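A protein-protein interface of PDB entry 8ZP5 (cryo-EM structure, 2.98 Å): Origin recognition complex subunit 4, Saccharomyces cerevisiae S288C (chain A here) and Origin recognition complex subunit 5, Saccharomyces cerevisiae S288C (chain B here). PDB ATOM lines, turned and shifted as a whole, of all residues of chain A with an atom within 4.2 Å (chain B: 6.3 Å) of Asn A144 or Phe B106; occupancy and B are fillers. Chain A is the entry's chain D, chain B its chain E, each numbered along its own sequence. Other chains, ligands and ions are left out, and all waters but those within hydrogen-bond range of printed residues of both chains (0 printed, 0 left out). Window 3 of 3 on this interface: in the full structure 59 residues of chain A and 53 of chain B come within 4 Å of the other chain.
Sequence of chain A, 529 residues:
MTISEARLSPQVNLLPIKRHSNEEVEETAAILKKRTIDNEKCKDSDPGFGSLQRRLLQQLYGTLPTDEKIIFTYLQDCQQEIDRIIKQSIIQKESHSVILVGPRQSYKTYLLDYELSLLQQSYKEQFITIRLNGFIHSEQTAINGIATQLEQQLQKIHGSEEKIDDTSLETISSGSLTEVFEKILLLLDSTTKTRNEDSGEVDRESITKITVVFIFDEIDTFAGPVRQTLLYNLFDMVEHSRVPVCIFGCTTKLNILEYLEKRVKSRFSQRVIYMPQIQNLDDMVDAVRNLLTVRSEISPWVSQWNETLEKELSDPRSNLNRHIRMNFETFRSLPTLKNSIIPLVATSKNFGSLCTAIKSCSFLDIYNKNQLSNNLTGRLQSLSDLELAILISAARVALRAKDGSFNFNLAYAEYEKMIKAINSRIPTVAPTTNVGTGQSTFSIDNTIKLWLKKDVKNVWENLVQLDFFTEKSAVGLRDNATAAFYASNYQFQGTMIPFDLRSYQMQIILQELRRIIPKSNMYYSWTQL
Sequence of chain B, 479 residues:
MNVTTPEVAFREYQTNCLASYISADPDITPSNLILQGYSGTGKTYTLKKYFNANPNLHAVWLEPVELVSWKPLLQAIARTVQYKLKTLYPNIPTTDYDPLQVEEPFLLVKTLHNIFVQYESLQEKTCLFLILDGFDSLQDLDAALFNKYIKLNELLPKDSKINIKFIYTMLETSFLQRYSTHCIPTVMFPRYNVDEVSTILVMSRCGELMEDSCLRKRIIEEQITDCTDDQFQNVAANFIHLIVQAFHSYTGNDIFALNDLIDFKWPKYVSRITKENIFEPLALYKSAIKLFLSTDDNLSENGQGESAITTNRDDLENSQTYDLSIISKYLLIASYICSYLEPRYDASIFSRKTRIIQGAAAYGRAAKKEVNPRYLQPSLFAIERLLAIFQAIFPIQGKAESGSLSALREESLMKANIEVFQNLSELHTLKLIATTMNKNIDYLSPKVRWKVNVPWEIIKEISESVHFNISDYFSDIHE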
ATOM      1  N   ILE A 136      28.457 -12.457 -19.272  1.00  0.00           N
ATOM      2  CA  ILE A 136      29.130 -13.121 -18.161  1.00  0.00           C
ATOM      3  C   ILE A 136      29.367 -14.600 -18.416  1.00  0.00           C
ATOM      4  O   ILE A 136      30.000 -15.266 -17.586  1.00  0.00           O
ATOM      5  CB  ILE A 136      28.350 -12.932 -16.847  1.00  0.00           C
ATOM      6  CG1 ILE A 136      26.995 -13.627 -16.916  1.00  0.00           C
ATOM      7  CG2 ILE A 136      28.135 -11.465 -16.561  1.00  0.00           C
ATOM      8  CD1 ILE A 136      26.292 -13.669 -15.587  1.00  0.00           C
ATOM      9  N   HIS A 137      28.887 -15.136 -19.532  1.00  0.00           N
ATOM     10  CA  HIS A 137      29.103 -16.530 -19.888  1.00  0.00           C
ATOM     11  C   HIS A 137      30.049 -16.615 -21.077  1.00  0.00           C
ATOM     12  O   HIS A 137      29.969 -15.807 -22.006  1.00  0.00           O
ATOM     13  CB  HIS A 137      27.785 -17.232 -20.224  1.00  0.00           C
ATOM     14  CG  HIS A 137      27.016 -17.681 -19.021  1.00  0.00           C
ATOM     15  ND1 HIS A 137      27.181 -18.926 -18.454  1.00  0.00           N
ATOM     16  CD2 HIS A 137      26.073 -17.054 -18.280  1.00  0.00           C
ATOM     17  CE1 HIS A 137      26.376 -19.045 -17.414  1.00  0.00           C
ATOM     18  NE2 HIS A 137      25.691 -17.923 -17.288  1.00  0.00           N
ATOM     19  N   GLN A 140      33.140 -21.902 -23.129  1.00  0.00           N
ATOM     20  CA  GLN A 140      33.371 -23.022 -22.223  1.00  0.00           C
ATOM     21  C   GLN A 140      32.468 -22.932 -21.001  1.00  0.00           C
ATOM     22  O   GLN A 140      31.984 -23.952 -20.498  1.00  0.00           O
ATOM     23  CB  GLN A 140      34.838 -23.060 -21.792  1.00  0.00           C
ATOM     24  CG  GLN A 140      35.816 -23.511 -22.868  1.00  0.00           C
ATOM     25  CD  GLN A 140      35.969 -22.500 -23.986  1.00  0.00           C
ATOM     26  OE1 GLN A 140      35.687 -22.795 -25.147  1.00  0.00           O
ATOM     27  NE2 GLN A 140      36.414 -21.299 -23.640  1.00  0.00           N
ATOM     28  N   THR A 141      32.234 -21.716 -20.511  1.00  0.00           N
ATOM     29  CA  THR A 141      31.501 -21.497 -19.273  1.00  0.00           C
ATOM     30  C   THR A 141      29.997 -21.709 -19.428  1.00  0.00           C
ATOM     31  O   THR A 141      29.323 -22.050 -18.448  1.00  0.00           O
ATOM     32  CB  THR A 141      31.794 -20.081 -18.769  1.00  0.00           C
ATOM     33  OG1 THR A 141      33.203 -19.934 -18.561  1.00  0.00           O
ATOM     34  CG2 THR A 141      31.102 -19.821 -17.466  1.00  0.00           C
ATOM     35  N   ALA A 142      29.461 -21.528 -20.638  1.00  0.00           N
ATOM     36  CA  ALA A 142      28.030 -21.709 -20.843  1.00  0.00           C
ATOM     37  C   ALA A 142      27.604 -23.150 -20.604  1.00  0.00           C
ATOM     38  O   ALA A 142      26.486 -23.390 -20.140  1.00  0.00           O
ATOM     39  CB  ALA A 142      27.637 -21.269 -22.251  1.00  0.00           C
ATOM     40  N   ILE A 143      28.468 -24.117 -20.914  1.00  0.00           N
ATOM     41  CA  ILE A 143      28.137 -25.519 -20.667  1.00  0.00           C
ATOM     42  C   ILE A 143      27.974 -25.770 -19.172  1.00  0.00           C
ATOM     43  O   ILE A 143      27.019 -26.422 -18.731  1.00  0.00           O
ATOM     44  CB  ILE A 143      29.209 -26.438 -21.278  1.00  0.00           C
ATOM     45  CG1 ILE A 143      29.631 -25.923 -22.653  1.00  0.00           C
ATOM     46  CG2 ILE A 143      28.693 -27.856 -21.377  1.00  0.00           C
ATOM     47  CD1 ILE A 143      28.522 -25.940 -23.678  1.00  0.00           C
ATOM     48  N   ASN A 144      28.908 -25.251 -18.371  1.00  0.00           N
ATOM     49  CA  ASN A 144      28.800 -25.387 -16.922  1.00  0.00           C
ATOM     50  C   ASN A 144      27.558 -24.682 -16.400  1.00  0.00           C
ATOM     51  O   ASN A 144      26.871 -25.198 -15.509  1.00  0.00           O
ATOM     52  CB  ASN A 144      30.052 -24.832 -16.247  1.00  0.00           C
ATOM     53  CG  ASN A 144      31.311 -25.563 -16.660  1.00  0.00           C
ATOM     54  OD1 ASN A 144      31.325 -26.788 -16.766  1.00  0.00           O
ATOM     55  ND2 ASN A 144      32.381 -24.814 -16.893  1.00  0.00           N
ATOM     56  N   GLY A 145      27.258 -23.497 -16.935  1.00  0.00           N
ATOM     57  CA  GLY A 145      26.057 -22.793 -16.515  1.00  0.00           C
ATOM     58  C   GLY A 145      24.796 -23.581 -16.806  1.00  0.00           C
ATOM     59  O   GLY A 145      23.909 -23.701 -15.955  1.00  0.00           O
ATOM     60  N   ILE A 146      24.708 -24.147 -18.012  1.00  0.00           N
ATOM     61  CA  ILE A 146      23.549 -24.952 -18.383  1.00  0.00           C
ATOM     62  C   ILE A 146      23.425 -26.162 -17.470  1.00  0.00           C
ATOM     63  O   ILE A 146      22.334 -26.483 -16.994  1.00  0.00           O
ATOM     64  CB  ILE A 146      23.632 -25.370 -19.862  1.00  0.00           C
ATOM     65  CG1 ILE A 146      23.519 -24.152 -20.775  1.00  0.00           C
ATOM     66  CG2 ILE A 146      22.543 -26.372 -20.196  1.00  0.00           C
ATOM     67  CD1 ILE A 146      23.680 -24.479 -22.239  1.00  0.00           C
ATOM     68  N   ALA A 147      24.538 -26.852 -17.209  1.00  0.00           N
ATOM     69  CA  ALA A 147      24.481 -28.048 -16.374  1.00  0.00           C
ATOM     70  C   ALA A 147      24.035 -27.715 -14.955  1.00  0.00           C
ATOM     71  O   ALA A 147      23.169 -28.394 -14.385  1.00  0.00           O
ATOM     72  CB  ALA A 147      25.840 -28.743 -16.361  1.00  0.00           C
ATOM     73  N   THR A 148      24.617 -26.665 -14.367  1.00  0.00           N
ATOM     74  CA  THR A 148      24.251 -26.290 -13.006  1.00  0.00           C
ATOM     75  C   THR A 148      22.792 -25.861 -12.925  1.00  0.00           C
ATOM     76  O   THR A 148      22.081 -26.228 -11.981  1.00  0.00           O
ATOM     77  CB  THR A 148      25.163 -25.176 -12.495  1.00  0.00           C
ATOM     78  OG1 THR A 148      25.224 -24.123 -13.462  1.00  0.00           O
ATOM     79  CG2 THR A 148      26.563 -25.707 -12.248  1.00  0.00           C
ATOM     80  N   LEU A 177      34.652 -30.715 -18.796  1.00  0.00           N
ATOM     81  CA  LEU A 177      33.755 -30.044 -19.732  1.00  0.00           C
ATOM     82  C   LEU A 177      33.225 -31.015 -20.778  1.00  0.00           C
ATOM     83  O   LEU A 177      32.066 -30.917 -21.195  1.00  0.00           O
ATOM     84  CB  LEU A 177      34.471 -28.872 -20.397  1.00  0.00           C
ATOM     85  CG  LEU A 177      33.572 -27.716 -20.832  1.00  0.00           C
ATOM     86  CD1 LEU A 177      32.832 -27.145 -19.639  1.00  0.00           C
ATOM     87  CD2 LEU A 177      34.393 -26.643 -21.517  1.00  0.00           C
ATOM     88  N   GLU B 104      35.674 -16.983 -12.767  1.00  0.00           N
ATOM     89  CA  GLU B 104      34.888 -16.494 -13.886  1.00  0.00           C
ATOM     90  C   GLU B 104      33.683 -15.754 -13.330  1.00  0.00           C
ATOM     91  O   GLU B 104      33.281 -15.989 -12.186  1.00  0.00           O
ATOM     92  CB  GLU B 104      34.434 -17.640 -14.800  1.00  0.00           C
ATOM     93  CG  GLU B 104      35.566 -18.351 -15.523  1.00  0.00           C
ATOM     94  CD  GLU B 104      36.261 -17.462 -16.535  1.00  0.00           C
ATOM     95  OE1 GLU B 104      35.591 -16.585 -17.119  1.00  0.00           O
ATOM     96  OE2 GLU B 104      37.479 -17.639 -16.747  1.00  0.00           O
ATOM     97  N   PRO B 105      33.098 -14.836 -14.106  1.00  0.00           N
ATOM     98  CA  PRO B 105      31.881 -14.159 -13.623  1.00  0.00           C
ATOM     99  C   PRO B 105      30.751 -15.122 -13.306  1.00  0.00           C
ATOM    100  O   PRO B 105      30.005 -14.907 -12.342  1.00  0.00           O
ATOM    101  CB  PRO B 105      31.526 -13.216 -14.780  1.00  0.00           C
ATOM    102  CG  PRO B 105      32.811 -13.001 -15.499  1.00  0.00           C
ATOM    103  CD  PRO B 105      33.558 -14.292 -15.394  1.00  0.00           C
ATOM    104  N   PHE B 106      30.608 -16.191 -14.094  1.00  0.00           N
ATOM    105  CA  PHE B 106      29.631 -17.220 -13.761  1.00  0.00           C
ATOM    106  C   PHE B 106      29.974 -17.916 -12.455  1.00  0.00           C
ATOM    107  O   PHE B 106      29.072 -18.303 -11.705  1.00  0.00           O
ATOM    108  CB  PHE B 106      29.531 -18.246 -14.884  1.00  0.00           C
ATOM    109  CG  PHE B 106      28.993 -19.575 -14.438  1.00  0.00           C
ATOM    110  CD1 PHE B 106      27.655 -19.725 -14.120  1.00  0.00           C
ATOM    111  CD2 PHE B 106      29.831 -20.672 -14.321  1.00  0.00           C
ATOM    112  CE1 PHE B 106      27.161 -20.943 -13.703  1.00  0.00           C
ATOM    113  CE2 PHE B 106      29.343 -21.892 -13.906  1.00  0.00           C
ATOM    114  CZ  PHE B 106      28.007 -22.028 -13.596  1.00  0.00           C
ATOM    115  N   LEU B 107      31.262 -18.111 -12.174  1.00  0.00           N
ATOM    116  CA  LEU B 107      31.641 -18.692 -10.893  1.00  0.00           C
ATOM    117  C   LEU B 107      31.259 -17.769  -9.744  1.00  0.00           C
ATOM    118  O   LEU B 107      30.836 -18.236  -8.682  1.00  0.00           O
ATOM    119  CB  LEU B 107      33.135 -19.003 -10.874  1.00  0.00           C
ATOM    120  CG  LEU B 107      33.516 -20.296 -11.597  1.00  0.00           C
ATOM    121  CD1 LEU B 107      34.971 -20.272 -12.023  1.00  0.00           C
ATOM    122  CD2 LEU B 107      33.233 -21.497 -10.714  1.00  0.00           C
ATOM    123  N   LEU B 108      31.386 -16.455  -9.943  1.00  0.00           N
ATOM    124  CA  LEU B 108      30.897 -15.512  -8.944  1.00  0.00           C
ATOM    125  C   LEU B 108      29.389 -15.624  -8.774  1.00  0.00           C
ATOM    126  O   LEU B 108      28.881 -15.584  -7.649  1.00  0.00           O
ATOM    127  CB  LEU B 108      31.282 -14.084  -9.326  1.00  0.00           C
ATOM    128  CG  LEU B 108      30.723 -13.003  -8.397  1.00  0.00           C
ATOM    129  CD1 LEU B 108      31.332 -13.122  -7.010  1.00  0.00           C
ATOM    130  CD2 LEU B 108      30.951 -11.615  -8.967  1.00  0.00           C
ATOM    131  N   VAL B 109      28.657 -15.767  -9.881  1.00  0.00           N
ATOM    132  CA  VAL B 109      27.204 -15.910  -9.800  1.00  0.00           C
ATOM    133  C   VAL B 109      26.839 -17.160  -9.008  1.00  0.00           C
ATOM    134  O   VAL B 109      25.964 -17.133  -8.134  1.00  0.00           O
ATOM    135  CB  VAL B 109      26.587 -15.938 -11.209  1.00  0.00           C
ATOM    136  CG1 VAL B 109      25.165 -16.467 -11.160  1.00  0.00           C
ATOM    137  CG2 VAL B 109      26.618 -14.554 -11.826  1.00  0.00           C
ATOM    138  N   LYS B 110      27.511 -18.273  -9.302  1.00  0.00           N
ATOM    139  CA  LYS B 110      27.229 -19.529  -8.614  1.00  0.00           C
ATOM    140  C   LYS B 110      27.575 -19.445  -7.132  1.00  0.00           C
ATOM    141  O   LYS B 110      26.815 -19.927  -6.285  1.00  0.00           O
ATOM    142  CB  LYS B 110      27.995 -20.669  -9.282  1.00  0.00           C
ATOM    143  CG  LYS B 110      27.754 -22.028  -8.656  1.00  0.00           C
ATOM    144  CD  LYS B 110      28.197 -23.148  -9.583  1.00  0.00           C
ATOM    145  CE  LYS B 110      29.655 -23.000  -9.979  1.00  0.00           C
ATOM    146  NZ  LYS B 110      30.565 -23.245  -8.828  1.00  0.00           N
ATOM    147  N   THR B 111      28.719 -18.842  -6.799  1.00  0.00           N
ATOM    148  CA  THR B 111      29.099 -18.704  -5.397  1.00  0.00           C
ATOM    149  C   THR B 111      28.120 -17.811  -4.647  1.00  0.00           C
ATOM    150  O   THR B 111      27.745 -18.111  -3.508  1.00  0.00           O
ATOM    151  CB  THR B 111      30.520 -18.153  -5.290  1.00  0.00           C
ATOM    152  OG1 THR B 111      31.415 -18.991  -6.030  1.00  0.00           O
ATOM    153  CG2 THR B 111      30.966 -18.110  -3.839  1.00  0.00           C
ATOM    154  N   LEU B 152      24.893  -8.755 -13.937  1.00  0.00           N
ATOM    155  CA  LEU B 152      25.131  -9.757 -12.901  1.00  0.00           C
ATOM    156  C   LEU B 152      23.896 -10.012 -12.044  1.00  0.00           C
ATOM    157  O   LEU B 152      23.689 -11.140 -11.586  1.00  0.00           O
ATOM    158  CB  LEU B 152      26.293  -9.320 -12.012  1.00  0.00           C
ATOM    159  CG  LEU B 152      27.046 -10.429 -11.280  1.00  0.00           C
ATOM    160  CD1 LEU B 152      27.924 -11.194 -12.252  1.00  0.00           C
ATOM    161  CD2 LEU B 152      27.870  -9.854 -10.142  1.00  0.00           C
ATOM    162  N   LEU B 155      20.927 -12.964 -13.219  1.00  0.00           N
ATOM    163  CA  LEU B 155      21.026 -14.412 -13.081  1.00  0.00           C
ATOM    164  C   LEU B 155      20.881 -14.885 -11.642  1.00  0.00           C
ATOM    165  O   LEU B 155      20.600 -16.068 -11.421  1.00  0.00           O
ATOM    166  CB  LEU B 155      22.353 -14.918 -13.653  1.00  0.00           C
ATOM    167  CG  LEU B 155      22.450 -15.030 -15.179  1.00  0.00           C
ATOM    168  CD1 LEU B 155      22.569 -13.669 -15.850  1.00  0.00           C
ATOM    169  CD2 LEU B 155      23.584 -15.950 -15.590  1.00  0.00           C
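O of Asn A144 lies within hydrogen-bond range of OG1 of Thr A148.
OG1 of Thr A148 is in hydrogen-bond range of O of Gly A145 (2.8 Å).
Ile A136 touches Pro B105.
Phe B106 touches Ile A136 (N to O, 3.7 Å).
Ile A136 touches Val B109.
Leu B155 touches Ile A136.
His A137 touches Phe B106.
NE2 of His A137 touches CD2 of Leu B155, at 3.3 Å.
CG2 of Thr A141 touches CB of Phe B106 (3.4 Å).
Phe B106 touches Asn A144 (CE2 to CB, 3.8 Å).
Phe B106 touches Gly A145 (CE1 to CA, 3.5 Å).
Phe B106 touches Thr A148 (CZ to OG1, 3.5 Å).
Of the 12 printed residues of chain A, 6 touch a printed residue of chain B.
Hydrophobic or aromatic side chains of chain A within 4 Å of the printed part of chain B: Ile A136 and His A137.
Of the 10 printed residues of chain B, 4 touch a printed residue of chain A.
Hydrophobic or aromatic side chains of chain B that line the printed part of chain A: Pro B105, Phe B106, Val B109 and Leu B155.
Of the printed residues of chain B, His A137 touches Phe B106 (3.6 Å) and Leu B155 (3.3 Å).
Of the printed residues of chain B, Thr A141 touches Phe B106 (3.4 Å).
Asn A144 touches just one residue of chain B: Phe B106 (3.8 Å).
Ile A146 touches none of the printed residues of chain B.
Of chain A, only Ile A136 (3.7 Å), His A137 (3.6 Å), Thr A141 (3.4 Å), Asn A144 (3.8 Å), Gly A145 (3.5 Å) and Thr A148 (3.5 Å) come within 4 Å of Phe B106.
Leu B107 touches none of the printed residues of chain A.
Printed residues of chain A within 4 Å of Val B109: Ile A136.
Of the printed residues of chain A, Leu B155 touches Ile A136 and His A137.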
